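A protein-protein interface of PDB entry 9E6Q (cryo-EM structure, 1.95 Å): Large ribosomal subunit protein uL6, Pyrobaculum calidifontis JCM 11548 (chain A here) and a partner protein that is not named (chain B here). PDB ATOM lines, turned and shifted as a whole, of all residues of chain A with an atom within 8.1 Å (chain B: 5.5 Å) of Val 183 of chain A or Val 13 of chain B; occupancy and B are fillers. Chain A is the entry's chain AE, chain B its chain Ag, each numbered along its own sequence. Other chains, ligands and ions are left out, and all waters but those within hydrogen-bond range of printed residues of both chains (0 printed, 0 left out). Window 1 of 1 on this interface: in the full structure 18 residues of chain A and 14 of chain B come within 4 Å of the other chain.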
ATOM      1  N   VAL A  96      10.147   2.710 -22.772  1.00  0.00           N
ATOM      2  CA  VAL A  96       9.519   2.415 -21.491  1.00  0.00           C
ATOM      3  C   VAL A  96      10.033   3.411 -20.462  1.00  0.00           C
ATOM      4  O   VAL A  96      11.241   3.513 -20.235  1.00  0.00           O
ATOM      5  CB  VAL A  96       9.799   0.972 -21.054  1.00  0.00           C
ATOM      6  CG1 VAL A  96       9.128   0.689 -19.726  1.00  0.00           C
ATOM      7  CG2 VAL A  96       9.326   0.005 -22.112  1.00  0.00           C
ATOM      8  N   ILE A  97       9.120   4.143 -19.839  1.00  0.00           N
ATOM      9  CA  ILE A  97       9.461   5.173 -18.871  1.00  0.00           C
ATOM     10  C   ILE A  97       8.747   4.863 -17.567  1.00  0.00           C
ATOM     11  O   ILE A  97       7.523   4.696 -17.550  1.00  0.00           O
ATOM     12  CB  ILE A  97       9.075   6.574 -19.379  1.00  0.00           C
ATOM     13  CG1 ILE A  97       9.829   6.893 -20.670  1.00  0.00           C
ATOM     14  CG2 ILE A  97       9.340   7.619 -18.320  1.00  0.00           C
ATOM     15  CD1 ILE A  97       9.515   8.242 -21.241  1.00  0.00           C
ATOM     16  N   TYR A  98       9.505   4.794 -16.475  1.00  0.00           N
ATOM     17  CA  TYR A  98       8.928   4.555 -15.162  1.00  0.00           C
ATOM     18  C   TYR A  98       9.578   5.476 -14.144  1.00  0.00           C
ATOM     19  O   TYR A  98      10.716   5.917 -14.319  1.00  0.00           O
ATOM     20  CB  TYR A  98       9.068   3.084 -14.742  1.00  0.00           C
ATOM     21  CG  TYR A  98      10.481   2.618 -14.478  1.00  0.00           C
ATOM     22  CD1 TYR A  98      11.120   2.904 -13.283  1.00  0.00           C
ATOM     23  CD2 TYR A  98      11.169   1.883 -15.425  1.00  0.00           C
ATOM     24  CE1 TYR A  98      12.401   2.480 -13.044  1.00  0.00           C
ATOM     25  CE2 TYR A  98      12.450   1.454 -15.195  1.00  0.00           C
ATOM     26  CZ  TYR A  98      13.063   1.756 -14.004  1.00  0.00           C
ATOM     27  OH  TYR A  98      14.347   1.328 -13.772  1.00  0.00           O
ATOM     28  N   THR A  99       8.843   5.755 -13.072  1.00  0.00           N
ATOM     29  CA  THR A  99       9.315   6.616 -11.998  1.00  0.00           C
ATOM     30  C   THR A  99       9.839   5.831 -10.803  1.00  0.00           C
ATOM     31  O   THR A  99      10.984   6.029 -10.393  1.00  0.00           O
ATOM     32  CB  THR A  99       8.197   7.563 -11.550  1.00  0.00           C
ATOM     33  OG1 THR A  99       6.968   6.839 -11.427  1.00  0.00           O
ATOM     34  CG2 THR A  99       8.017   8.676 -12.559  1.00  0.00           C
ATOM     35  N   HIS A 100       9.034   4.942 -10.235  1.00  0.00           N
ATOM     36  CA  HIS A 100       9.471   4.153  -9.092  1.00  0.00           C
ATOM     37  C   HIS A 100       9.422   2.656  -9.337  1.00  0.00           C
ATOM     38  O   HIS A 100      10.346   1.947  -8.942  1.00  0.00           O
ATOM     39  CB  HIS A 100       8.624   4.494  -7.856  1.00  0.00           C
ATOM     40  CG  HIS A 100       8.971   3.691  -6.643  1.00  0.00           C
ATOM     41  ND1 HIS A 100       8.475   2.426  -6.417  1.00  0.00           N
ATOM     42  CD2 HIS A 100       9.776   3.971  -5.592  1.00  0.00           C
ATOM     43  CE1 HIS A 100       8.955   1.964  -5.278  1.00  0.00           C
ATOM     44  NE2 HIS A 100       9.747   2.883  -4.757  1.00  0.00           N
ATOM     45  N   MET A 103       8.914  -1.460 -14.905  1.00  0.00           N
ATOM     46  CA  MET A 103       8.074  -2.342 -15.696  1.00  0.00           C
ATOM     47  C   MET A 103       8.885  -3.503 -16.248  1.00  0.00           C
ATOM     48  O   MET A 103      10.061  -3.364 -16.586  1.00  0.00           O
ATOM     49  CB  MET A 103       7.428  -1.581 -16.850  1.00  0.00           C
ATOM     50  CG  MET A 103       6.107  -0.940 -16.505  1.00  0.00           C
ATOM     51  SD  MET A 103       5.484   0.071 -17.854  1.00  0.00           S
ATOM     52  CE  MET A 103       6.214   1.647 -17.438  1.00  0.00           C
ATOM     53  N   PHE A 117       3.540  -2.446 -13.850  1.00  0.00           N
ATOM     54  CA  PHE A 117       3.240  -1.068 -14.212  1.00  0.00           C
ATOM     55  C   PHE A 117       2.637  -0.346 -13.019  1.00  0.00           C
ATOM     56  O   PHE A 117       1.553  -0.710 -12.557  1.00  0.00           O
ATOM     57  CB  PHE A 117       2.285  -0.995 -15.401  1.00  0.00           C
ATOM     58  CG  PHE A 117       1.868   0.401 -15.742  1.00  0.00           C
ATOM     59  CD1 PHE A 117       2.814   1.371 -16.002  1.00  0.00           C
ATOM     60  CD2 PHE A 117       0.535   0.755 -15.778  1.00  0.00           C
ATOM     61  CE1 PHE A 117       2.438   2.657 -16.308  1.00  0.00           C
ATOM     62  CE2 PHE A 117       0.159   2.042 -16.082  1.00  0.00           C
ATOM     63  CZ  PHE A 117       1.111   2.992 -16.345  1.00  0.00           C
ATOM     64  N   LEU A 118       3.340   0.658 -12.506  1.00  0.00           N
ATOM     65  CA  LEU A 118       2.937   1.396 -11.315  1.00  0.00           C
ATOM     66  C   LEU A 118       2.746   0.488 -10.111  1.00  0.00           C
ATOM     67  O   LEU A 118       1.986   0.819  -9.202  1.00  0.00           O
ATOM     68  CB  LEU A 118       1.662   2.205 -11.558  1.00  0.00           C
ATOM     69  CG  LEU A 118       1.688   3.266 -12.650  1.00  0.00           C
ATOM     70  CD1 LEU A 118       0.291   3.805 -12.868  1.00  0.00           C
ATOM     71  CD2 LEU A 118       2.624   4.375 -12.272  1.00  0.00           C
ATOM     72  N   THR A 163      -1.127   1.624 -21.320  1.00  0.00           N
ATOM     73  CA  THR A 163      -0.482   2.187 -20.146  1.00  0.00           C
ATOM     74  C   THR A 163      -1.003   3.572 -19.792  1.00  0.00           C
ATOM     75  O   THR A 163      -0.447   4.221 -18.904  1.00  0.00           O
ATOM     76  CB  THR A 163       1.029   2.239 -20.353  1.00  0.00           C
ATOM     77  OG1 THR A 163       1.335   3.174 -21.391  1.00  0.00           O
ATOM     78  CG2 THR A 163       1.547   0.876 -20.740  1.00  0.00           C
ATOM     79  N   PRO A 171      -3.640   9.252 -13.026  1.00  0.00           N
ATOM     80  CA  PRO A 171      -2.823  10.035 -12.098  1.00  0.00           C
ATOM     81  C   PRO A 171      -2.666  11.475 -12.562  1.00  0.00           C
ATOM     82  O   PRO A 171      -2.819  11.802 -13.739  1.00  0.00           O
ATOM     83  CB  PRO A 171      -1.482   9.304 -12.117  1.00  0.00           C
ATOM     84  CG  PRO A 171      -1.424   8.695 -13.459  1.00  0.00           C
ATOM     85  CD  PRO A 171      -2.822   8.381 -13.883  1.00  0.00           C
ATOM     86  N   SER A 172      -2.358  12.334 -11.606  1.00  0.00           N
ATOM     87  CA  SER A 172      -2.133  13.736 -11.917  1.00  0.00           C
ATOM     88  C   SER A 172      -0.855  13.877 -12.735  1.00  0.00           C
ATOM     89  O   SER A 172       0.195  13.376 -12.325  1.00  0.00           O
ATOM     90  CB  SER A 172      -2.042  14.557 -10.640  1.00  0.00           C
ATOM     91  OG  SER A 172      -1.590  15.868 -10.910  1.00  0.00           O
ATOM     92  N   PRO A 173      -0.907  14.522 -13.901  1.00  0.00           N
ATOM     93  CA  PRO A 173       0.299  14.637 -14.729  1.00  0.00           C
ATOM     94  C   PRO A 173       1.378  15.492 -14.099  1.00  0.00           C
ATOM     95  O   PRO A 173       2.563  15.267 -14.364  1.00  0.00           O
ATOM     96  CB  PRO A 173      -0.228  15.268 -16.024  1.00  0.00           C
ATOM     97  CG  PRO A 173      -1.686  15.032 -15.999  1.00  0.00           C
ATOM     98  CD  PRO A 173      -2.073  15.114 -14.566  1.00  0.00           C
ATOM     99  N   HIS A 174       1.009  16.471 -13.286  1.00  0.00           N
ATOM    100  CA  HIS A 174       1.961  17.359 -12.649  1.00  0.00           C
ATOM    101  C   HIS A 174       2.026  17.072 -11.158  1.00  0.00           C
ATOM    102  O   HIS A 174       1.045  16.647 -10.547  1.00  0.00           O
ATOM    103  CB  HIS A 174       1.601  18.828 -12.889  1.00  0.00           C
ATOM    104  CG  HIS A 174       0.373  19.284 -12.169  1.00  0.00           C
ATOM    105  ND1 HIS A 174       0.358  19.585 -10.824  1.00  0.00           N
ATOM    106  CD2 HIS A 174      -0.887  19.501 -12.614  1.00  0.00           C
ATOM    107  CE1 HIS A 174      -0.856  19.965 -10.471  1.00  0.00           C
ATOM    108  NE2 HIS A 174      -1.631  19.921 -11.540  1.00  0.00           N
ATOM    109  N   GLY A 175       3.195  17.314 -10.578  1.00  0.00           N
ATOM    110  CA  GLY A 175       3.419  17.078  -9.171  1.00  0.00           C
ATOM    111  C   GLY A 175       2.927  18.222  -8.312  1.00  0.00           C
ATOM    112  O   GLY A 175       2.232  19.133  -8.764  1.00  0.00           O
ATOM    113  N   GLY A 179       5.676  20.468 -10.468  1.00  0.00           N
ATOM    114  CA  GLY A 179       6.688  19.622 -11.058  1.00  0.00           C
ATOM    115  C   GLY A 179       6.083  18.478 -11.849  1.00  0.00           C
ATOM    116  O   GLY A 179       4.871  18.356 -12.023  1.00  0.00           O
ATOM    117  N   LEU A 180       6.966  17.625 -12.354  1.00  0.00           N
ATOM    118  CA  LEU A 180       6.521  16.412 -13.021  1.00  0.00           C
ATOM    119  C   LEU A 180       5.788  15.509 -12.040  1.00  0.00           C
ATOM    120  O   LEU A 180       6.230  15.313 -10.907  1.00  0.00           O
ATOM    121  CB  LEU A 180       7.712  15.677 -13.625  1.00  0.00           C
ATOM    122  CG  LEU A 180       7.489  15.004 -14.975  1.00  0.00           C
ATOM    123  CD1 LEU A 180       6.971  15.972 -16.015  1.00  0.00           C
ATOM    124  CD2 LEU A 180       8.776  14.371 -15.431  1.00  0.00           C
ATOM    125  N   GLY A 181       4.662  14.966 -12.477  1.00  0.00           N
ATOM    126  CA  GLY A 181       3.886  14.037 -11.684  1.00  0.00           C
ATOM    127  C   GLY A 181       4.252  12.597 -11.973  1.00  0.00           C
ATOM    128  O   GLY A 181       5.330  12.292 -12.483  1.00  0.00           O
ATOM    129  N   VAL A 182       3.326  11.695 -11.653  1.00  0.00           N
ATOM    130  CA  VAL A 182       3.530  10.274 -11.923  1.00  0.00           C
ATOM    131  C   VAL A 182       3.305  10.075 -13.417  1.00  0.00           C
ATOM    132  O   VAL A 182       2.174   9.925 -13.874  1.00  0.00           O
ATOM    133  CB  VAL A 182       2.604   9.386 -11.087  1.00  0.00           C
ATOM    134  CG1 VAL A 182       2.747   7.937 -11.503  1.00  0.00           C
ATOM    135  CG2 VAL A 182       2.912   9.532  -9.612  1.00  0.00           C
ATOM    136  N   VAL A 183       4.388  10.099 -14.187  1.00  0.00           N
ATOM    137  CA  VAL A 183       4.298   9.895 -15.624  1.00  0.00           C
ATOM    138  C   VAL A 183       5.035   8.612 -15.970  1.00  0.00           C
ATOM    139  O   VAL A 183       6.215   8.630 -16.333  1.00  0.00           O
ATOM    140  CB  VAL A 183       4.873  11.101 -16.388  1.00  0.00           C
ATOM    141  CG1 VAL A 183       3.870  12.234 -16.405  1.00  0.00           C
ATOM    142  CG2 VAL A 183       6.170  11.571 -15.753  1.00  0.00           C
ATOM    143  N   ASP A 184       4.342   7.493 -15.888  1.00  0.00           N
ATOM    144  CA  ASP A 184       4.902   6.203 -16.246  1.00  0.00           C
ATOM    145  C   ASP A 184       4.137   5.686 -17.443  1.00  0.00           C
ATOM    146  O   ASP A 184       2.938   5.941 -17.578  1.00  0.00           O
ATOM    147  CB  ASP A 184       4.810   5.198 -15.097  1.00  0.00           C
ATOM    148  CG  ASP A 184       5.658   5.586 -13.909  1.00  0.00           C
ATOM    149  OD1 ASP A 184       5.688   6.779 -13.561  1.00  0.00           O
ATOM    150  OD2 ASP A 184       6.289   4.693 -13.314  1.00  0.00           O
ATOM    151  N   GLY A 185       4.824   4.977 -18.314  1.00  0.00           N
ATOM    152  CA  GLY A 185       4.154   4.395 -19.452  1.00  0.00           C
ATOM    153  C   GLY A 185       5.137   4.034 -20.537  1.00  0.00           C
ATOM    154  O   GLY A 185       6.348   4.160 -20.389  1.00  0.00           O
ATOM    155  N   ILE A 186       4.569   3.562 -21.635  1.00  0.00           N
ATOM    156  CA  ILE A 186       5.298   3.253 -22.850  1.00  0.00           C
ATOM    157  C   ILE A 186       4.839   4.237 -23.909  1.00  0.00           C
ATOM    158  O   ILE A 186       3.637   4.376 -24.155  1.00  0.00           O
ATOM    159  CB  ILE A 186       5.063   1.799 -23.281  1.00  0.00           C
ATOM    160  CG1 ILE A 186       5.198   0.886 -22.064  1.00  0.00           C
ATOM    161  CG2 ILE A 186       6.038   1.395 -24.354  1.00  0.00           C
ATOM    162  CD1 ILE A 186       4.840  -0.535 -22.331  1.00  0.00           C
ATOM    163  N   TYR A 187       5.787   4.936 -24.515  1.00  0.00           N
ATOM    164  CA  TYR A 187       5.491   6.010 -25.447  1.00  0.00           C
ATOM    165  C   TYR A 187       6.104   5.674 -26.795  1.00  0.00           C
ATOM    166  O   TYR A 187       7.286   5.332 -26.871  1.00  0.00           O
ATOM    167  CB  TYR A 187       6.033   7.337 -24.924  1.00  0.00           C
ATOM    168  CG  TYR A 187       5.476   7.742 -23.586  1.00  0.00           C
ATOM    169  CD1 TYR A 187       4.280   8.428 -23.489  1.00  0.00           C
ATOM    170  CD2 TYR A 187       6.137   7.419 -22.416  1.00  0.00           C
ATOM    171  CE1 TYR A 187       3.772   8.797 -22.267  1.00  0.00           C
ATOM    172  CE2 TYR A 187       5.633   7.776 -21.192  1.00  0.00           C
ATOM    173  CZ  TYR A 187       4.454   8.464 -21.122  1.00  0.00           C
ATOM    174  OH  TYR A 187       3.956   8.822 -19.900  1.00  0.00           O
ATOM    175  N   VAL A 189       7.973   6.603 -29.862  1.00  0.00           N
ATOM    176  CA  VAL A 189       8.967   7.656 -29.994  1.00  0.00           C
ATOM    177  C   VAL A 189       9.336   7.951 -31.438  1.00  0.00           C
ATOM    178  O   VAL A 189       9.948   8.997 -31.698  1.00  0.00           O
ATOM    179  CB  VAL A 189      10.233   7.328 -29.180  1.00  0.00           C
ATOM    180  CG1 VAL A 189       9.884   7.233 -27.726  1.00  0.00           C
ATOM    181  CG2 VAL A 189      10.839   6.036 -29.647  1.00  0.00           C
ATOM    182  N   ILE B   3      10.328  13.336  -8.397  1.00  0.00           N
ATOM    183  CA  ILE B   3      10.157  12.641  -9.665  1.00  0.00           C
ATOM    184  C   ILE B   3      11.023  13.305 -10.727  1.00  0.00           C
ATOM    185  O   ILE B   3      10.724  14.404 -11.183  1.00  0.00           O
ATOM    186  CB  ILE B   3       8.676  12.611 -10.075  1.00  0.00           C
ATOM    187  CG1 ILE B   3       7.869  11.808  -9.054  1.00  0.00           C
ATOM    188  CG2 ILE B   3       8.515  12.031 -11.467  1.00  0.00           C
ATOM    189  CD1 ILE B   3       6.444  11.528  -9.466  1.00  0.00           C
ATOM    190  N   LEU B   5      13.411  12.795 -14.368  1.00  0.00           N
ATOM    191  CA  LEU B   5      13.764  12.048 -15.565  1.00  0.00           C
ATOM    192  C   LEU B   5      14.906  12.760 -16.272  1.00  0.00           C
ATOM    193  O   LEU B   5      15.029  13.985 -16.189  1.00  0.00           O
ATOM    194  CB  LEU B   5      12.569  11.915 -16.512  1.00  0.00           C
ATOM    195  CG  LEU B   5      11.334  11.194 -15.978  1.00  0.00           C
ATOM    196  CD1 LEU B   5      10.163  11.402 -16.910  1.00  0.00           C
ATOM    197  CD2 LEU B   5      11.607   9.716 -15.793  1.00  0.00           C
ATOM    198  N   LYS B   9      14.094  11.416 -21.763  1.00  0.00           N
ATOM    199  CA  LYS B   9      12.774  10.954 -21.365  1.00  0.00           C
ATOM    200  C   LYS B   9      11.849  12.107 -21.013  1.00  0.00           C
ATOM    201  O   LYS B   9      10.636  12.006 -21.225  1.00  0.00           O
ATOM    202  CB  LYS B   9      12.889   9.996 -20.185  1.00  0.00           C
ATOM    203  CG  LYS B   9      13.446   8.648 -20.562  1.00  0.00           C
ATOM    204  CD  LYS B   9      13.640   7.779 -19.348  1.00  0.00           C
ATOM    205  CE  LYS B   9      14.266   6.459 -19.733  1.00  0.00           C
ATOM    206  NZ  LYS B   9      14.607   5.650 -18.542  1.00  0.00           N
ATOM    207  N   LEU B  10      12.389  13.197 -20.469  1.00  0.00           N
ATOM    208  CA  LEU B  10      11.550  14.349 -20.164  1.00  0.00           C
ATOM    209  C   LEU B  10      10.953  14.943 -21.431  1.00  0.00           C
ATOM    210  O   LEU B  10       9.792  15.364 -21.441  1.00  0.00           O
ATOM    211  CB  LEU B  10      12.353  15.398 -19.401  1.00  0.00           C
ATOM    212  CG  LEU B  10      11.615  16.703 -19.120  1.00  0.00           C
ATOM    213  CD1 LEU B  10      10.698  16.531 -17.927  1.00  0.00           C
ATOM    214  CD2 LEU B  10      12.601  17.828 -18.878  1.00  0.00           C
ATOM    215  N   ALA B  11      11.732  14.986 -22.512  1.00  0.00           N
ATOM    216  CA  ALA B  11      11.215  15.506 -23.772  1.00  0.00           C
ATOM    217  C   ALA B  11      10.099  14.626 -24.317  1.00  0.00           C
ATOM    218  O   ALA B  11       9.103  15.133 -24.840  1.00  0.00           O
ATOM    219  CB  ALA B  11      12.345  15.632 -24.791  1.00  0.00           C
ATOM    220  N   ILE B  12      10.251  13.306 -24.202  1.00  0.00           N
ATOM    221  CA  ILE B  12       9.203  12.393 -24.646  1.00  0.00           C
ATOM    222  C   ILE B  12       7.925  12.621 -23.856  1.00  0.00           C
ATOM    223  O   ILE B  12       6.828  12.674 -24.420  1.00  0.00           O
ATOM    224  CB  ILE B  12       9.682  10.938 -24.519  1.00  0.00           C
ATOM    225  CG1 ILE B  12      10.867  10.679 -25.439  1.00  0.00           C
ATOM    226  CG2 ILE B  12       8.559   9.984 -24.821  1.00  0.00           C
ATOM    227  CD1 ILE B  12      11.415   9.291 -25.318  1.00  0.00           C
ATOM    228  N   VAL B  13       8.047  12.757 -22.537  1.00  0.00           N
ATOM    229  CA  VAL B  13       6.873  12.892 -21.687  1.00  0.00           C
ATOM    230  C   VAL B  13       6.169  14.214 -21.955  1.00  0.00           C
ATOM    231  O   VAL B  13       4.935  14.277 -21.996  1.00  0.00           O
ATOM    232  CB  VAL B  13       7.277  12.739 -20.211  1.00  0.00           C
ATOM    233  CG1 VAL B  13       6.274  13.410 -19.300  1.00  0.00           C
ATOM    234  CG2 VAL B  13       7.415  11.280 -19.860  1.00  0.00           C
ATOM    235  N   LEU B  14       6.938  15.288 -22.145  1.00  0.00           N
ATOM    236  CA  LEU B  14       6.336  16.586 -22.427  1.00  0.00           C
ATOM    237  C   LEU B  14       5.563  16.561 -23.736  1.00  0.00           C
ATOM    238  O   LEU B  14       4.464  17.114 -23.826  1.00  0.00           O
ATOM    239  CB  LEU B  14       7.405  17.673 -22.464  1.00  0.00           C
ATOM    240  CG  LEU B  14       8.010  18.098 -21.129  1.00  0.00           C
ATOM    241  CD1 LEU B  14       8.384  19.560 -21.174  1.00  0.00           C
ATOM    242  CD2 LEU B  14       7.059  17.827 -19.983  1.00  0.00           C
ATOM    243  N   GLN B  15       6.116  15.913 -24.760  1.00  0.00           N
ATOM    244  CA  GLN B  15       5.425  15.840 -26.039  1.00  0.00           C
ATOM    245  C   GLN B  15       4.108  15.086 -25.918  1.00  0.00           C
ATOM    246  O   GLN B  15       3.101  15.482 -26.512  1.00  0.00           O
ATOM    247  CB  GLN B  15       6.323  15.183 -27.080  1.00  0.00           C
ATOM    248  CG  GLN B  15       5.595  14.770 -28.332  1.00  0.00           C
ATOM    249  CD  GLN B  15       5.188  15.957 -29.181  1.00  0.00           C
ATOM    250  OE1 GLN B  15       5.827  17.009 -29.144  1.00  0.00           O
ATOM    251  NE2 GLN B  15       4.116  15.797 -29.947  1.00  0.00           N
ATOM    252  N   HIS B  16       4.091  14.001 -25.153  1.00  0.00           N
ATOM    253  CA  HIS B  16       2.920  13.139 -25.109  1.00  0.00           C
ATOM    254  C   HIS B  16       1.902  13.550 -24.058  1.00  0.00           C
ATOM    255  O   HIS B  16       0.716  13.245 -24.211  1.00  0.00           O
ATOM    256  CB  HIS B  16       3.349  11.694 -24.862  1.00  0.00           C
ATOM    257  CG  HIS B  16       3.921  11.025 -26.069  1.00  0.00           C
ATOM    258  ND1 HIS B  16       3.185  10.184 -26.873  1.00  0.00           N
ATOM    259  CD2 HIS B  16       5.154  11.087 -26.622  1.00  0.00           C
ATOM    260  CE1 HIS B  16       3.943   9.747 -27.860  1.00  0.00           C
ATOM    261  NE2 HIS B  16       5.142  10.282 -27.733  1.00  0.00           N
ATOM    262  N   ARG B  17       2.321  14.239 -23.001  1.00  0.00           N
ATOM    263  CA  ARG B  17       1.420  14.565 -21.909  1.00  0.00           C
ATOM    264  C   ARG B  17       1.180  16.055 -21.722  1.00  0.00           C
ATOM    265  O   ARG B  17       0.285  16.420 -20.957  1.00  0.00           O
ATOM    266  CB  ARG B  17       1.945  13.976 -20.591  1.00  0.00           C
ATOM    267  CG  ARG B  17       2.200  12.488 -20.632  1.00  0.00           C
ATOM    268  CD  ARG B  17       0.913  11.711 -20.722  1.00  0.00           C
ATOM    269  NE  ARG B  17       1.121  10.282 -20.538  1.00  0.00           N
ATOM    270  CZ  ARG B  17       1.063   9.656 -19.372  1.00  0.00           C
ATOM    271  NH1 ARG B  17       0.795  10.304 -18.253  1.00  0.00           N
ATOM    272  NH2 ARG B  17       1.282   8.347 -19.329  1.00  0.00           N
ATOM    273  N   PHE B  18       1.937  16.923 -22.393  1.00  0.00           N
ATOM    274  CA  PHE B  18       1.826  18.349 -22.115  1.00  0.00           C
ATOM    275  C   PHE B  18       1.864  19.214 -23.369  1.00  0.00           C
ATOM    276  O   PHE B  18       2.171  20.406 -23.272  1.00  0.00           O
ATOM    277  CB  PHE B  18       2.945  18.806 -21.182  1.00  0.00           C
ATOM    278  CG  PHE B  18       2.935  18.135 -19.849  1.00  0.00           C
ATOM    279  CD1 PHE B  18       2.209  18.659 -18.803  1.00  0.00           C
ATOM    280  CD2 PHE B  18       3.652  16.974 -19.643  1.00  0.00           C
ATOM    281  CE1 PHE B  18       2.202  18.042 -17.577  1.00  0.00           C
ATOM    282  CE2 PHE B  18       3.643  16.355 -18.424  1.00  0.00           C
ATOM    283  CZ  PHE B  18       2.919  16.891 -17.387  1.00  0.00           C
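CD1 of Ile 97 of chain A touches O of Lys 9 of chain B, at 3.9 Å.
CD1 of Ile 97 of chain A touches CG2 of Val 13 of chain B (3.9 Å).
Ile 3 of chain B touches Thr 99 of chain A.
Phe 18 of chain B touches Pro 173 of chain A (CZ to O, 3.5 Å).
Leu 180 of chain A touches Leu 10 of chain B (CD2 to CD1, 3.8 Å).
Ile 3 of chain B touches Gly 181 of chain A.
Ile 3 of chain B touches Val 182 of chain A (CD1 to N, 3.8 Å).
CG1 of Val 183 of chain A touches CG1 of Val 13 of chain B, at 3.9 Å.
Tyr 187 of chain A touches Ile 12 of chain B (CB to CG2, 3.7 Å).
Val 189 of chain A touches Ile 12 of chain B.
Of the printed residues of chain B, Gly 181 of chain A touches Ile 3.
Printed residues of chain B within 4 Å of Val 183 of chain A: Val 13 (3.9 Å).
Ile 186 of chain A touches none of the printed residues of chain B.
Of the printed residues of chain B, Val 189 of chain A touches Ile 12 (3.5 Å).
Of chain A, only Ile 97 and Val 183 come within 4 Å of Val 13 of chain B.
Of the printed residues of chain A, Phe 18 of chain B touches Pro 173.
The nearest residue of chain B that does not touch Val 183 of chain A is Arg 17 of chain B (4.1 Å).
NH2 of Arg 17 of chain B lies within hydrogen-bond range of OH of Tyr 187 of chain A.
O of Asp 184 of chain A is in hydrogen-bond range of NH2 of Arg 17 of chain B, at 3.4 Å.
N of Gly 185 of chain A lies within hydrogen-bond range of O of Ile 97 of chain A, 2.8 Å away.
The side-chain hydroxyl of Thr 99 of chain A lies within hydrogen-bond range of the side-chain carboxylate of Asp 184 of chain A (2.5 Å).
The backbone NH of Gly 181 of chain A lies within hydrogen-bond range of the backbone carbonyl oxygen of Pro 173 of chain A, 2.8 Å away.
Of the 24 printed residues of chain A, 10 touch a printed residue of chain B.
Hydrophobic or aromatic side chains of chain A that line the printed part of chain B: Ile 97, Pro 173, Leu 180, Val 183, Tyr 187 and Val 189.
Of the 12 printed residues of chain B, 9 touch a printed residue of chain A.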
